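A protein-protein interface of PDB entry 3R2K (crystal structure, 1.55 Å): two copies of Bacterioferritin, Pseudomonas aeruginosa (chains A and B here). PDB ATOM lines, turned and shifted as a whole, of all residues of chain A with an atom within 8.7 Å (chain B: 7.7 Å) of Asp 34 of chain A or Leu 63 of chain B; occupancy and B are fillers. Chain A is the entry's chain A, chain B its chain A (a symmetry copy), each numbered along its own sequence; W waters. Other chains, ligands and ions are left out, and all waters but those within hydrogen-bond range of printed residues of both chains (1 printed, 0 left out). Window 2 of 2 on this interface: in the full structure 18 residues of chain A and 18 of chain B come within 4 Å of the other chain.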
ATOM      1  N   PHE A  26     -30.970  33.107  10.957  1.00  0.00           N
ATOM      2  CA  PHE A  26     -31.488  32.497  12.214  1.00  0.00           C
ATOM      3  C   PHE A  26     -30.645  31.266  12.547  1.00  0.00           C
ATOM      4  O   PHE A  26     -30.043  31.159  13.631  1.00  0.00           O
ATOM      5  CB  PHE A  26     -32.974  32.108  12.010  1.00  0.00           C
ATOM      6  CG  PHE A  26     -33.792  31.868  13.269  1.00  0.00           C
ATOM      7  CD1 PHE A  26     -35.153  31.621  13.129  1.00  0.00           C
ATOM      8  CD2 PHE A  26     -33.254  31.890  14.547  1.00  0.00           C
ATOM      9  CE1 PHE A  26     -35.958  31.410  14.214  1.00  0.00           C
ATOM     10  CE2 PHE A  26     -34.059  31.714  15.635  1.00  0.00           C
ATOM     11  CZ  PHE A  26     -35.408  31.457  15.480  1.00  0.00           C
ATOM     12  N   ILE A  27     -30.563  30.315  11.621  1.00  0.00           N
ATOM     13  CA  ILE A  27     -29.801  29.110  11.912  1.00  0.00           C
ATOM     14  C   ILE A  27     -28.311  29.377  12.032  1.00  0.00           C
ATOM     15  O   ILE A  27     -27.658  28.885  12.964  1.00  0.00           O
ATOM     16  CB  ILE A  27     -30.095  27.965  10.897  1.00  0.00           C
ATOM     17  CG1 ILE A  27     -29.299  26.713  11.263  1.00  0.00           C
ATOM     18  CG2 ILE A  27     -29.790  28.364   9.480  1.00  0.00           C
ATOM     19  CD1 ILE A  27     -29.532  26.192  12.660  1.00  0.00           C
ATOM     20  N   HIS A  28     -27.728  30.163  11.131  1.00  0.00           N
ATOM     21  CA  HIS A  28     -26.290  30.446  11.266  1.00  0.00           C
ATOM     22  C   HIS A  28     -25.939  31.155  12.567  1.00  0.00           C
ATOM     23  O   HIS A  28     -24.962  30.786  13.214  1.00  0.00           O
ATOM     24  CB  HIS A  28     -25.751  31.276  10.104  1.00  0.00           C
ATOM     25  CG  HIS A  28     -25.526  30.493   8.848  1.00  0.00           C
ATOM     26  ND1 HIS A  28     -25.271  31.096   7.635  1.00  0.00           N
ATOM     27  CD2 HIS A  28     -25.457  29.160   8.623  1.00  0.00           C
ATOM     28  CE1 HIS A  28     -25.087  30.164   6.710  1.00  0.00           C
ATOM     29  NE2 HIS A  28     -25.197  28.985   7.288  1.00  0.00           N
ATOM     30  N   SER A  29     -26.720  32.154  12.959  1.00  0.00           N
ATOM     31  CA  SER A  29     -26.377  32.860  14.187  1.00  0.00           C
ATOM     32  C   SER A  29     -26.397  31.910  15.376  1.00  0.00           C
ATOM     33  O   SER A  29     -25.500  31.949  16.232  1.00  0.00           O
ATOM     34  CB  SER A  29     -27.306  34.042  14.413  1.00  0.00           C
ATOM     35  OG  SER A  29     -28.647  33.647  14.542  1.00  0.00           O
ATOM     36  N   ARG A  30     -27.397  31.037  15.448  1.00  0.00           N
ATOM     37  CA  ARG A  30     -27.471  30.120  16.573  1.00  0.00           C
ATOM     38  C   ARG A  30     -26.389  29.043  16.506  1.00  0.00           C
ATOM     39  O   ARG A  30     -25.939  28.574  17.553  1.00  0.00           O
ATOM     40  CB  ARG A  30     -28.868  29.513  16.673  1.00  0.00           C
ATOM     41  CG  ARG A  30     -29.841  30.369  17.464  1.00  0.00           C
ATOM     42  CD  ARG A  30     -30.056  31.741  16.853  1.00  0.00           C
ATOM     43  NE  ARG A  30     -31.073  32.474  17.600  1.00  0.00           N
ATOM     44  CZ  ARG A  30     -31.298  33.771  17.448  1.00  0.00           C
ATOM     45  NH1 ARG A  30     -30.610  34.457  16.552  1.00  0.00           N
ATOM     46  NH2 ARG A  30     -32.247  34.374  18.154  1.00  0.00           N
ATOM     47  N   MET A  31     -25.960  28.645  15.305  1.00  0.00           N
ATOM     48  CA  MET A  31     -24.827  27.726  15.180  1.00  0.00           C
ATOM     49  C   MET A  31     -23.540  28.373  15.689  1.00  0.00           C
ATOM     50  O   MET A  31     -22.750  27.743  16.375  1.00  0.00           O
ATOM     51  CB  MET A  31     -24.658  27.285  13.718  1.00  0.00           C
ATOM     52  CG  MET A  31     -25.720  26.317  13.227  1.00  0.00           C
ATOM     53  SD  MET A  31     -25.580  26.012  11.456  1.00  0.00           S
ATOM     54  CE  MET A  31     -24.002  25.181  11.370  1.00  0.00           C
ATOM     55  N   TYR A  32     -23.317  29.637  15.342  1.00  0.00           N
ATOM     56  CA  TYR A  32     -22.163  30.370  15.810  1.00  0.00           C
ATOM     57  C   TYR A  32     -22.162  30.433  17.340  1.00  0.00           C
ATOM     58  O   TYR A  32     -21.106  30.267  17.965  1.00  0.00           O
ATOM     59  CB  TYR A  32     -22.181  31.774  15.234  1.00  0.00           C
ATOM     60  CG  TYR A  32     -21.842  31.892  13.770  1.00  0.00           C
ATOM     61  CD1 TYR A  32     -20.765  31.200  13.215  1.00  0.00           C
ATOM     62  CD2 TYR A  32     -22.539  32.759  12.958  1.00  0.00           C
ATOM     63  CE1 TYR A  32     -20.438  31.348  11.881  1.00  0.00           C
ATOM     64  CE2 TYR A  32     -22.209  32.923  11.606  1.00  0.00           C
ATOM     65  CZ  TYR A  32     -21.165  32.217  11.080  1.00  0.00           C
ATOM     66  OH  TYR A  32     -20.844  32.389   9.751  1.00  0.00           O
ATOM     67  N   GLU A  33     -23.330  30.667  17.944  1.00  0.00           N
ATOM     68  CA  GLU A  33     -23.439  30.699  19.419  1.00  0.00           C
ATOM     69  C   GLU A  33     -23.165  29.314  20.030  1.00  0.00           C
ATOM     70  O   GLU A  33     -22.499  29.209  21.062  1.00  0.00           O
ATOM     71  CB  GLU A  33     -24.807  31.246  19.851  1.00  0.00           C
ATOM     72  CG  GLU A  33     -24.997  31.386  21.369  1.00  0.00           C
ATOM     73  CD  GLU A  33     -23.946  32.258  22.064  1.00  0.00           C
ATOM     74  OE1 GLU A  33     -23.328  33.133  21.424  1.00  0.00           O
ATOM     75  OE2 GLU A  33     -23.737  32.054  23.283  1.00  0.00           O
ATOM     76  N   ASP A  34     -23.655  28.264  19.382  1.00  0.00           N
ATOM     77  CA  ASP A  34     -23.464  26.867  19.817  1.00  0.00           C
ATOM     78  C   ASP A  34     -21.963  26.557  19.929  1.00  0.00           C
ATOM     79  O   ASP A  34     -21.527  25.849  20.842  1.00  0.00           O
ATOM     80  CB  ASP A  34     -24.187  25.922  18.815  1.00  0.00           C
ATOM     81  CG  ASP A  34     -23.904  24.409  19.025  1.00  0.00           C
ATOM     82  OD1 ASP A  34     -24.162  23.893  20.119  1.00  0.00           O
ATOM     83  OD2 ASP A  34     -23.493  23.724  18.060  1.00  0.00           O
ATOM     84  N   TRP A  35     -21.171  27.131  19.033  1.00  0.00           N
ATOM     85  CA  TRP A  35     -19.736  26.895  19.016  1.00  0.00           C
ATOM     86  C   TRP A  35     -18.958  27.860  19.900  1.00  0.00           C
ATOM     87  O   TRP A  35     -17.750  27.717  20.058  1.00  0.00           O
ATOM     88  CB  TRP A  35     -19.219  27.003  17.586  1.00  0.00           C
ATOM     89  CG  TRP A  35     -19.697  25.934  16.712  1.00  0.00           C
ATOM     90  CD1 TRP A  35     -20.064  24.673  17.077  1.00  0.00           C
ATOM     91  CD2 TRP A  35     -19.853  26.005  15.291  1.00  0.00           C
ATOM     92  NE1 TRP A  35     -20.444  23.946  15.966  1.00  0.00           N
ATOM     93  CE2 TRP A  35     -20.331  24.750  14.860  1.00  0.00           C
ATOM     94  CE3 TRP A  35     -19.648  27.017  14.345  1.00  0.00           C
ATOM     95  CZ2 TRP A  35     -20.598  24.476  13.524  1.00  0.00           C
ATOM     96  CZ3 TRP A  35     -19.911  26.748  13.032  1.00  0.00           C
ATOM     97  CH2 TRP A  35     -20.378  25.484  12.627  1.00  0.00           C
ATOM     98  N   GLY A  36     -19.631  28.866  20.433  1.00  0.00           N
ATOM     99  CA  GLY A  36     -18.964  29.832  21.287  1.00  0.00           C
ATOM    100  C   GLY A  36     -18.427  31.080  20.622  1.00  0.00           C
ATOM    101  O   GLY A  36     -17.637  31.810  21.224  1.00  0.00           O
ATOM    102  N   PHE A  37     -18.882  31.380  19.405  1.00  0.00           N
ATOM    103  CA  PHE A  37     -18.450  32.603  18.721  1.00  0.00           C
ATOM    104  C   PHE A  37     -19.508  33.680  18.893  1.00  0.00           C
ATOM    105  O   PHE A  37     -20.331  33.924  17.999  1.00  0.00           O
ATOM    106  CB  PHE A  37     -18.208  32.309  17.236  1.00  0.00           C
ATOM    107  CG  PHE A  37     -17.135  31.290  17.005  1.00  0.00           C
ATOM    108  CD1 PHE A  37     -15.843  31.521  17.454  1.00  0.00           C
ATOM    109  CD2 PHE A  37     -17.415  30.108  16.359  1.00  0.00           C
ATOM    110  CE1 PHE A  37     -14.847  30.576  17.266  1.00  0.00           C
ATOM    111  CE2 PHE A  37     -16.422  29.146  16.175  1.00  0.00           C
ATOM    112  CZ  PHE A  37     -15.144  29.386  16.630  1.00  0.00           C
ATOM    113  N   SER A  38     -19.499  34.315  20.054  1.00  0.00           N
ATOM    114  CA  SER A  38     -20.606  35.191  20.375  1.00  0.00           C
ATOM    115  C   SER A  38     -20.611  36.448  19.503  1.00  0.00           C
ATOM    116  O   SER A  38     -21.668  37.009  19.261  1.00  0.00           O
ATOM    117  CB  SER A  38     -20.622  35.502  21.868  1.00  0.00           C
ATOM    118  OG  SER A  38     -20.982  34.323  22.579  1.00  0.00           O
ATOM    119  N   TYR A  41     -22.552  35.350  16.478  1.00  0.00           N
ATOM    120  CA  TYR A  41     -23.951  35.274  16.896  1.00  0.00           C
ATOM    121  C   TYR A  41     -24.585  36.661  16.883  1.00  0.00           C
ATOM    122  O   TYR A  41     -25.645  36.856  16.305  1.00  0.00           O
ATOM    123  CB  TYR A  41     -24.089  34.663  18.287  1.00  0.00           C
ATOM    124  CG  TYR A  41     -25.466  34.916  18.840  1.00  0.00           C
ATOM    125  CD1 TYR A  41     -25.699  35.996  19.674  1.00  0.00           C
ATOM    126  CD2 TYR A  41     -26.538  34.122  18.483  1.00  0.00           C
ATOM    127  CE1 TYR A  41     -26.970  36.261  20.163  1.00  0.00           C
ATOM    128  CE2 TYR A  41     -27.811  34.367  18.973  1.00  0.00           C
ATOM    129  CZ  TYR A  41     -28.018  35.439  19.809  1.00  0.00           C
ATOM    130  OH  TYR A  41     -29.294  35.692  20.286  1.00  0.00           O
ATOM    131  N   MET A  85     -20.241  28.924   6.113  1.00  0.00           N
ATOM    132  CA  MET A  85     -21.422  29.701   6.480  1.00  0.00           C
ATOM    133  C   MET A  85     -21.288  31.135   5.974  1.00  0.00           C
ATOM    134  O   MET A  85     -22.238  31.715   5.435  1.00  0.00           O
ATOM    135  CB  MET A  85     -21.576  29.665   7.996  1.00  0.00           C
ATOM    136  CG  MET A  85     -21.928  28.285   8.500  1.00  0.00           C
ATOM    137  SD  MET A  85     -21.459  28.026  10.207  1.00  0.00           S
ATOM    138  CE  MET A  85     -22.812  28.926  11.024  1.00  0.00           C
ATOM    139  N   MET B   1     -23.598  16.937  24.080  1.00  0.00           N
ATOM    140  CA  MET B   1     -24.273  15.695  24.528  1.00  0.00           C
ATOM    141  C   MET B   1     -25.200  15.263  23.412  1.00  0.00           C
ATOM    142  O   MET B   1     -26.010  16.044  22.960  1.00  0.00           O
ATOM    143  CB  MET B   1     -25.085  15.990  25.793  1.00  0.00           C
ATOM    144  CG  MET B   1     -25.897  14.822  26.332  1.00  0.00           C
ATOM    145  SD  MET B   1     -26.895  15.265  27.785  1.00  0.00           S
ATOM    146  CE  MET B   1     -28.015  16.477  27.096  1.00  0.00           C
ATOM    147  N   ILE B   8     -34.859  14.335  19.127  1.00  0.00           N
ATOM    148  CA  ILE B   8     -34.372  15.360  18.195  1.00  0.00           C
ATOM    149  C   ILE B   8     -35.296  15.485  16.987  1.00  0.00           C
ATOM    150  O   ILE B   8     -35.674  16.576  16.592  1.00  0.00           O
ATOM    151  CB  ILE B   8     -32.934  15.075  17.761  1.00  0.00           C
ATOM    152  CG1 ILE B   8     -31.977  15.228  18.949  1.00  0.00           C
ATOM    153  CG2 ILE B   8     -32.516  16.004  16.647  1.00  0.00           C
ATOM    154  CD1 ILE B   8     -30.557  14.632  18.704  1.00  0.00           C
ATOM    155  N   LEU B  11     -38.462  17.235  18.147  1.00  0.00           N
ATOM    156  CA  LEU B  11     -38.228  18.666  18.335  1.00  0.00           C
ATOM    157  C   LEU B  11     -38.185  19.381  16.986  1.00  0.00           C
ATOM    158  O   LEU B  11     -38.672  20.499  16.858  1.00  0.00           O
ATOM    159  CB  LEU B  11     -36.932  18.907  19.120  1.00  0.00           C
ATOM    160  CG  LEU B  11     -36.903  18.417  20.570  1.00  0.00           C
ATOM    161  CD1 LEU B  11     -35.538  18.632  21.157  1.00  0.00           C
ATOM    162  CD2 LEU B  11     -37.978  19.065  21.415  1.00  0.00           C
ATOM    163  N   ASN B  12     -37.577  18.753  15.981  1.00  0.00           N
ATOM    164  CA  ASN B  12     -37.552  19.343  14.651  1.00  0.00           C
ATOM    165  C   ASN B  12     -38.962  19.486  14.081  1.00  0.00           C
ATOM    166  O   ASN B  12     -39.250  20.466  13.412  1.00  0.00           O
ATOM    167  CB  ASN B  12     -36.659  18.509  13.733  1.00  0.00           C
ATOM    168  CG  ASN B  12     -35.261  19.053  13.635  1.00  0.00           C
ATOM    169  OD1 ASN B  12     -35.069  20.261  13.698  1.00  0.00           O
ATOM    170  ND2 ASN B  12     -34.281  18.182  13.428  1.00  0.00           N
ATOM    171  N   ASP B  56     -36.843  29.663  18.545  1.00  0.00           N
ATOM    172  CA  ASP B  56     -35.466  29.843  18.965  1.00  0.00           C
ATOM    173  C   ASP B  56     -35.102  28.837  20.063  1.00  0.00           C
ATOM    174  O   ASP B  56     -34.049  28.207  20.023  1.00  0.00           O
ATOM    175  CB  ASP B  56     -35.288  31.278  19.469  1.00  0.00           C
ATOM    176  CG  ASP B  56     -33.839  31.715  19.567  1.00  0.00           C
ATOM    177  OD1 ASP B  56     -32.914  31.035  19.063  1.00  0.00           O
ATOM    178  OD2 ASP B  56     -33.617  32.829  20.139  1.00  0.00           O
ATOM    179  N   ALA B  57     -35.976  28.688  21.055  1.00  0.00           N
ATOM    180  CA  ALA B  57     -35.694  27.749  22.138  1.00  0.00           C
ATOM    181  C   ALA B  57     -35.552  26.329  21.603  1.00  0.00           C
ATOM    182  O   ALA B  57     -34.656  25.593  22.014  1.00  0.00           O
ATOM    183  CB  ALA B  57     -36.769  27.806  23.208  1.00  0.00           C
ATOM    184  N   LEU B  58     -36.401  25.940  20.663  1.00  0.00           N
ATOM    185  CA  LEU B  58     -36.271  24.592  20.086  1.00  0.00           C
ATOM    186  C   LEU B  58     -35.007  24.419  19.279  1.00  0.00           C
ATOM    187  O   LEU B  58     -34.307  23.416  19.407  1.00  0.00           O
ATOM    188  CB  LEU B  58     -37.493  24.239  19.210  1.00  0.00           C
ATOM    189  CG  LEU B  58     -38.790  24.227  19.985  1.00  0.00           C
ATOM    190  CD1 LEU B  58     -39.954  23.992  19.032  1.00  0.00           C
ATOM    191  CD2 LEU B  58     -38.811  23.211  21.096  1.00  0.00           C
ATOM    192  N   LEU B  59     -34.716  25.394  18.436  1.00  0.00           N
ATOM    193  CA  LEU B  59     -33.536  25.371  17.593  1.00  0.00           C
ATOM    194  C   LEU B  59     -32.282  25.230  18.440  1.00  0.00           C
ATOM    195  O   LEU B  59     -31.422  24.384  18.164  1.00  0.00           O
ATOM    196  CB  LEU B  59     -33.533  26.663  16.771  1.00  0.00           C
ATOM    197  CG  LEU B  59     -32.558  26.840  15.621  1.00  0.00           C
ATOM    198  CD1 LEU B  59     -32.962  28.095  14.789  1.00  0.00           C
ATOM    199  CD2 LEU B  59     -31.155  26.929  16.158  1.00  0.00           C
ATOM    200  N   ARG B  60     -32.178  26.027  19.507  1.00  0.00           N
ATOM    201  CA  ARG B  60     -30.999  25.987  20.347  1.00  0.00           C
ATOM    202  C   ARG B  60     -30.913  24.669  21.094  1.00  0.00           C
ATOM    203  O   ARG B  60     -29.823  24.144  21.264  1.00  0.00           O
ATOM    204  CB  ARG B  60     -31.018  27.148  21.351  1.00  0.00           C
ATOM    205  CG  ARG B  60     -30.866  28.499  20.683  1.00  0.00           C
ATOM    206  CD  ARG B  60     -30.591  29.564  21.702  1.00  0.00           C
ATOM    207  NE  ARG B  60     -30.943  30.887  21.211  1.00  0.00           N
ATOM    208  CZ  ARG B  60     -30.262  32.002  21.434  1.00  0.00           C
ATOM    209  NH1 ARG B  60     -29.136  31.998  22.123  1.00  0.00           N
ATOM    210  NH2 ARG B  60     -30.740  33.139  20.973  1.00  0.00           N
ATOM    211  N   ARG B  61     -32.051  24.102  21.493  1.00  0.00           N
ATOM    212  CA  ARG B  61     -32.054  22.804  22.184  1.00  0.00           C
ATOM    213  C   ARG B  61     -31.589  21.700  21.243  1.00  0.00           C
ATOM    214  O   ARG B  61     -30.799  20.858  21.623  1.00  0.00           O
ATOM    215  CB  ARG B  61     -33.449  22.478  22.719  1.00  0.00           C
ATOM    216  CG  ARG B  61     -33.515  21.135  23.465  1.00  0.00           C
ATOM    217  CD  ARG B  61     -32.694  21.162  24.743  1.00  0.00           C
ATOM    218  NE  ARG B  61     -32.832  19.911  25.474  1.00  0.00           N
ATOM    219  CZ  ARG B  61     -32.051  19.526  26.474  1.00  0.00           C
ATOM    220  NH1 ARG B  61     -31.103  20.327  26.968  1.00  0.00           N
ATOM    221  NH2 ARG B  61     -32.241  18.331  26.994  1.00  0.00           N
ATOM    222  N   ILE B  62     -32.062  21.741  19.991  1.00  0.00           N
ATOM    223  CA  ILE B  62     -31.655  20.753  18.983  1.00  0.00           C
ATOM    224  C   ILE B  62     -30.156  20.828  18.759  1.00  0.00           C
ATOM    225  O   ILE B  62     -29.486  19.795  18.728  1.00  0.00           O
ATOM    226  CB  ILE B  62     -32.418  20.986  17.678  1.00  0.00           C
ATOM    227  CG1 ILE B  62     -33.872  20.588  17.852  1.00  0.00           C
ATOM    228  CG2 ILE B  62     -31.823  20.197  16.531  1.00  0.00           C
ATOM    229  CD1 ILE B  62     -34.861  21.305  16.901  1.00  0.00           C
ATOM    230  N   LEU B  63     -29.599  22.042  18.659  1.00  0.00           N
ATOM    231  CA  LEU B  63     -28.152  22.181  18.519  1.00  0.00           C
ATOM    232  C   LEU B  63     -27.373  21.625  19.711  1.00  0.00           C
ATOM    233  O   LEU B  63     -26.343  20.948  19.554  1.00  0.00           O
ATOM    234  CB  LEU B  63     -27.768  23.654  18.288  1.00  0.00           C
ATOM    235  CG  LEU B  63     -28.139  24.175  16.890  1.00  0.00           C
ATOM    236  CD1 LEU B  63     -27.892  25.672  16.875  1.00  0.00           C
ATOM    237  CD2 LEU B  63     -27.387  23.504  15.715  1.00  0.00           C
ATOM    238  N   LEU B  64     -27.861  21.913  20.919  1.00  0.00           N
ATOM    239  CA  LEU B  64     -27.203  21.461  22.138  1.00  0.00           C
ATOM    240  C   LEU B  64     -27.107  19.926  22.138  1.00  0.00           C
ATOM    241  O   LEU B  64     -26.113  19.355  22.592  1.00  0.00           O
ATOM    242  CB  LEU B  64     -27.954  21.974  23.355  1.00  0.00           C
ATOM    243  CG  LEU B  64     -27.431  21.540  24.738  1.00  0.00           C
ATOM    244  CD1 LEU B  64     -27.916  22.473  25.801  1.00  0.00           C
ATOM    245  CD2 LEU B  64     -27.880  20.155  25.058  1.00  0.00           C
ATOM    246  N   LEU B  65     -28.160  19.293  21.630  1.00  0.00           N
ATOM    247  CA  LEU B  65     -28.298  17.835  21.561  1.00  0.00           C
ATOM    248  C   LEU B  65     -27.579  17.257  20.334  1.00  0.00           C
ATOM    249  O   LEU B  65     -27.708  16.066  20.026  1.00  0.00           O
ATOM    250  CB  LEU B  65     -29.762  17.429  21.574  1.00  0.00           C
ATOM    251  CG  LEU B  65     -30.528  17.759  22.857  1.00  0.00           C
ATOM    252  CD1 LEU B  65     -31.976  17.383  22.721  1.00  0.00           C
ATOM    253  CD2 LEU B  65     -29.911  17.119  24.087  1.00  0.00           C
ATOM    254  N   GLU B  66     -26.832  18.106  19.635  1.00  0.00           N
ATOM    255  CA  GLU B  66     -26.002  17.697  18.511  1.00  0.00           C
ATOM    256  C   GLU B  66     -26.821  17.294  17.289  1.00  0.00           C
ATOM    257  O   GLU B  66     -26.351  16.566  16.408  1.00  0.00           O
ATOM    258  CB  GLU B  66     -24.995  16.617  18.931  1.00  0.00           C
ATOM    259  CG  GLU B  66     -24.165  17.090  20.127  1.00  0.00           C
ATOM    260  CD  GLU B  66     -22.997  16.216  20.459  1.00  0.00           C
ATOM    261  OE1 GLU B  66     -22.565  15.430  19.597  1.00  0.00           O
ATOM    262  OE2 GLU B  66     -22.508  16.331  21.601  1.00  0.00           O
ATOM    263  N   GLY B  67     -28.046  17.795  17.223  1.00  0.00           N
ATOM    264  CA  GLY B  67     -28.869  17.603  16.052  1.00  0.00           C
ATOM    265  C   GLY B  67     -28.735  18.728  15.064  1.00  0.00           C
ATOM    266  O   GLY B  67     -28.082  19.746  15.308  1.00  0.00           O
ATOM    267  N   THR B  68     -29.355  18.529  13.918  1.00  0.00           N
ATOM    268  CA  THR B  68     -29.359  19.516  12.854  1.00  0.00           C
ATOM    269  C   THR B  68     -30.772  20.076  12.683  1.00  0.00           C
ATOM    270  O   THR B  68     -31.713  19.353  12.312  1.00  0.00           O
ATOM    271  CB  THR B  68     -28.920  18.867  11.527  1.00  0.00           C
ATOM    272  OG1 THR B  68     -27.600  18.322  11.661  1.00  0.00           O
ATOM    273  CG2 THR B  68     -28.939  19.887  10.404  1.00  0.00           C
ATOM    274  N   PRO B  69     -30.959  21.376  12.968  1.00  0.00           N
ATOM    275  CA  PRO B  69     -32.316  21.908  12.871  1.00  0.00           C
ATOM    276  C   PRO B  69     -32.888  21.925  11.462  1.00  0.00           C
ATOM    277  O   PRO B  69     -32.195  22.219  10.498  1.00  0.00           O
ATOM    278  CB  PRO B  69     -32.175  23.346  13.410  1.00  0.00           C
ATOM    279  CG  PRO B  69     -30.989  23.277  14.331  1.00  0.00           C
ATOM    280  CD  PRO B  69     -30.046  22.325  13.640  1.00  0.00           C
HETATM  281  O   HOH W   1     -24.480  21.191  17.574  1.00  0.00           O
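The guanidinium group (NE) of Arg 30 of chain A lies within salt-bridge range of the side-chain carboxylate (OD1) of Asp 56 of chain B, at 2.8 Å.
The guanidinium group (NH2) of Arg 30 of chain A lies close to the guanidinium group (NH2) of Arg 60 of chain B (3.4 Å).
OH of Tyr 41 of chain A is in hydrogen-bond range of NH2 of Arg 60 of chain B (3.0 Å).
The backbone carbonyl oxygen of Phe 26 of chain A is in hydrogen-bond range of the side-chain hydroxyl of Ser 29 of chain A, 3.0 Å away.
OG of Ser 29 of chain A sits at hydrogen-bond distance from NH1 of Arg 30 of chain A (2.9 Å).
OD1 of Asp 56 of chain B is in salt-bridge range of NE of Arg 60 of chain B (2.9 Å).
Asp 56 of chain B touches Phe 26 of chain A.
Phe 26 of chain A touches Leu 59 of chain B.
CD1 of Ile 27 of chain A touches CD2 of Leu 59 of chain B (3.9 Å).
CD1 of Ile 27 of chain A touches CG of Pro 69 of chain B, 3.7 Å away.
Arg 30 of chain A touches Leu 59 of chain B (CB to CD2, 3.5 Å).
Arg 30 of chain A touches Leu 63 of chain B.
Met 31 of chain A touches Leu 63 of chain B.
OD1 of Asp 34 of chain A touches O of Leu 63 of chain B, at 3.7 Å.
Asp 34 of chain A touches one residue of chain B.
Phe 37 of chain A touches none of the printed residues of chain B.
Of the printed residues of chain A, Asp 56 of chain B touches Phe 26 and Arg 30.
Leu 58 of chain B touches none of the printed residues of chain A.
Printed residues of chain A within 4 Å of Leu 59 of chain B: Phe 26 (3.8 Å), Ile 27 (3.9 Å) and Arg 30 (3.5 Å).
Of the printed residues of chain A, Arg 60 of chain B touches Arg 30 and Tyr 41.
Leu 63 of chain B touches just these residues of chain A: Arg 30 (3.6 Å), Met 31 (3.9 Å) and Asp 34 (3.7 Å).
Printed residues of chain A within 4 Å of Pro 69 of chain B: Ile 27.
Of the 15 printed residues of chain A, 6 touch a printed residue of chain B.
Along chain A the printed residues that touch a printed residue of chain B span positions 26 to 41.
Among the printed residues, 11 pairs touch across the chains.
No position is printed for both chains.
Of the 11 pairs that touch across the chains among the printed residues, none has its exchanged pair printed and touching as well.
Water W1 lies within hydrogen-bond range of O of Leu 63 of chain B (2.7 Å) and OD2 of Asp 34 of chain A (2.8 Å).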
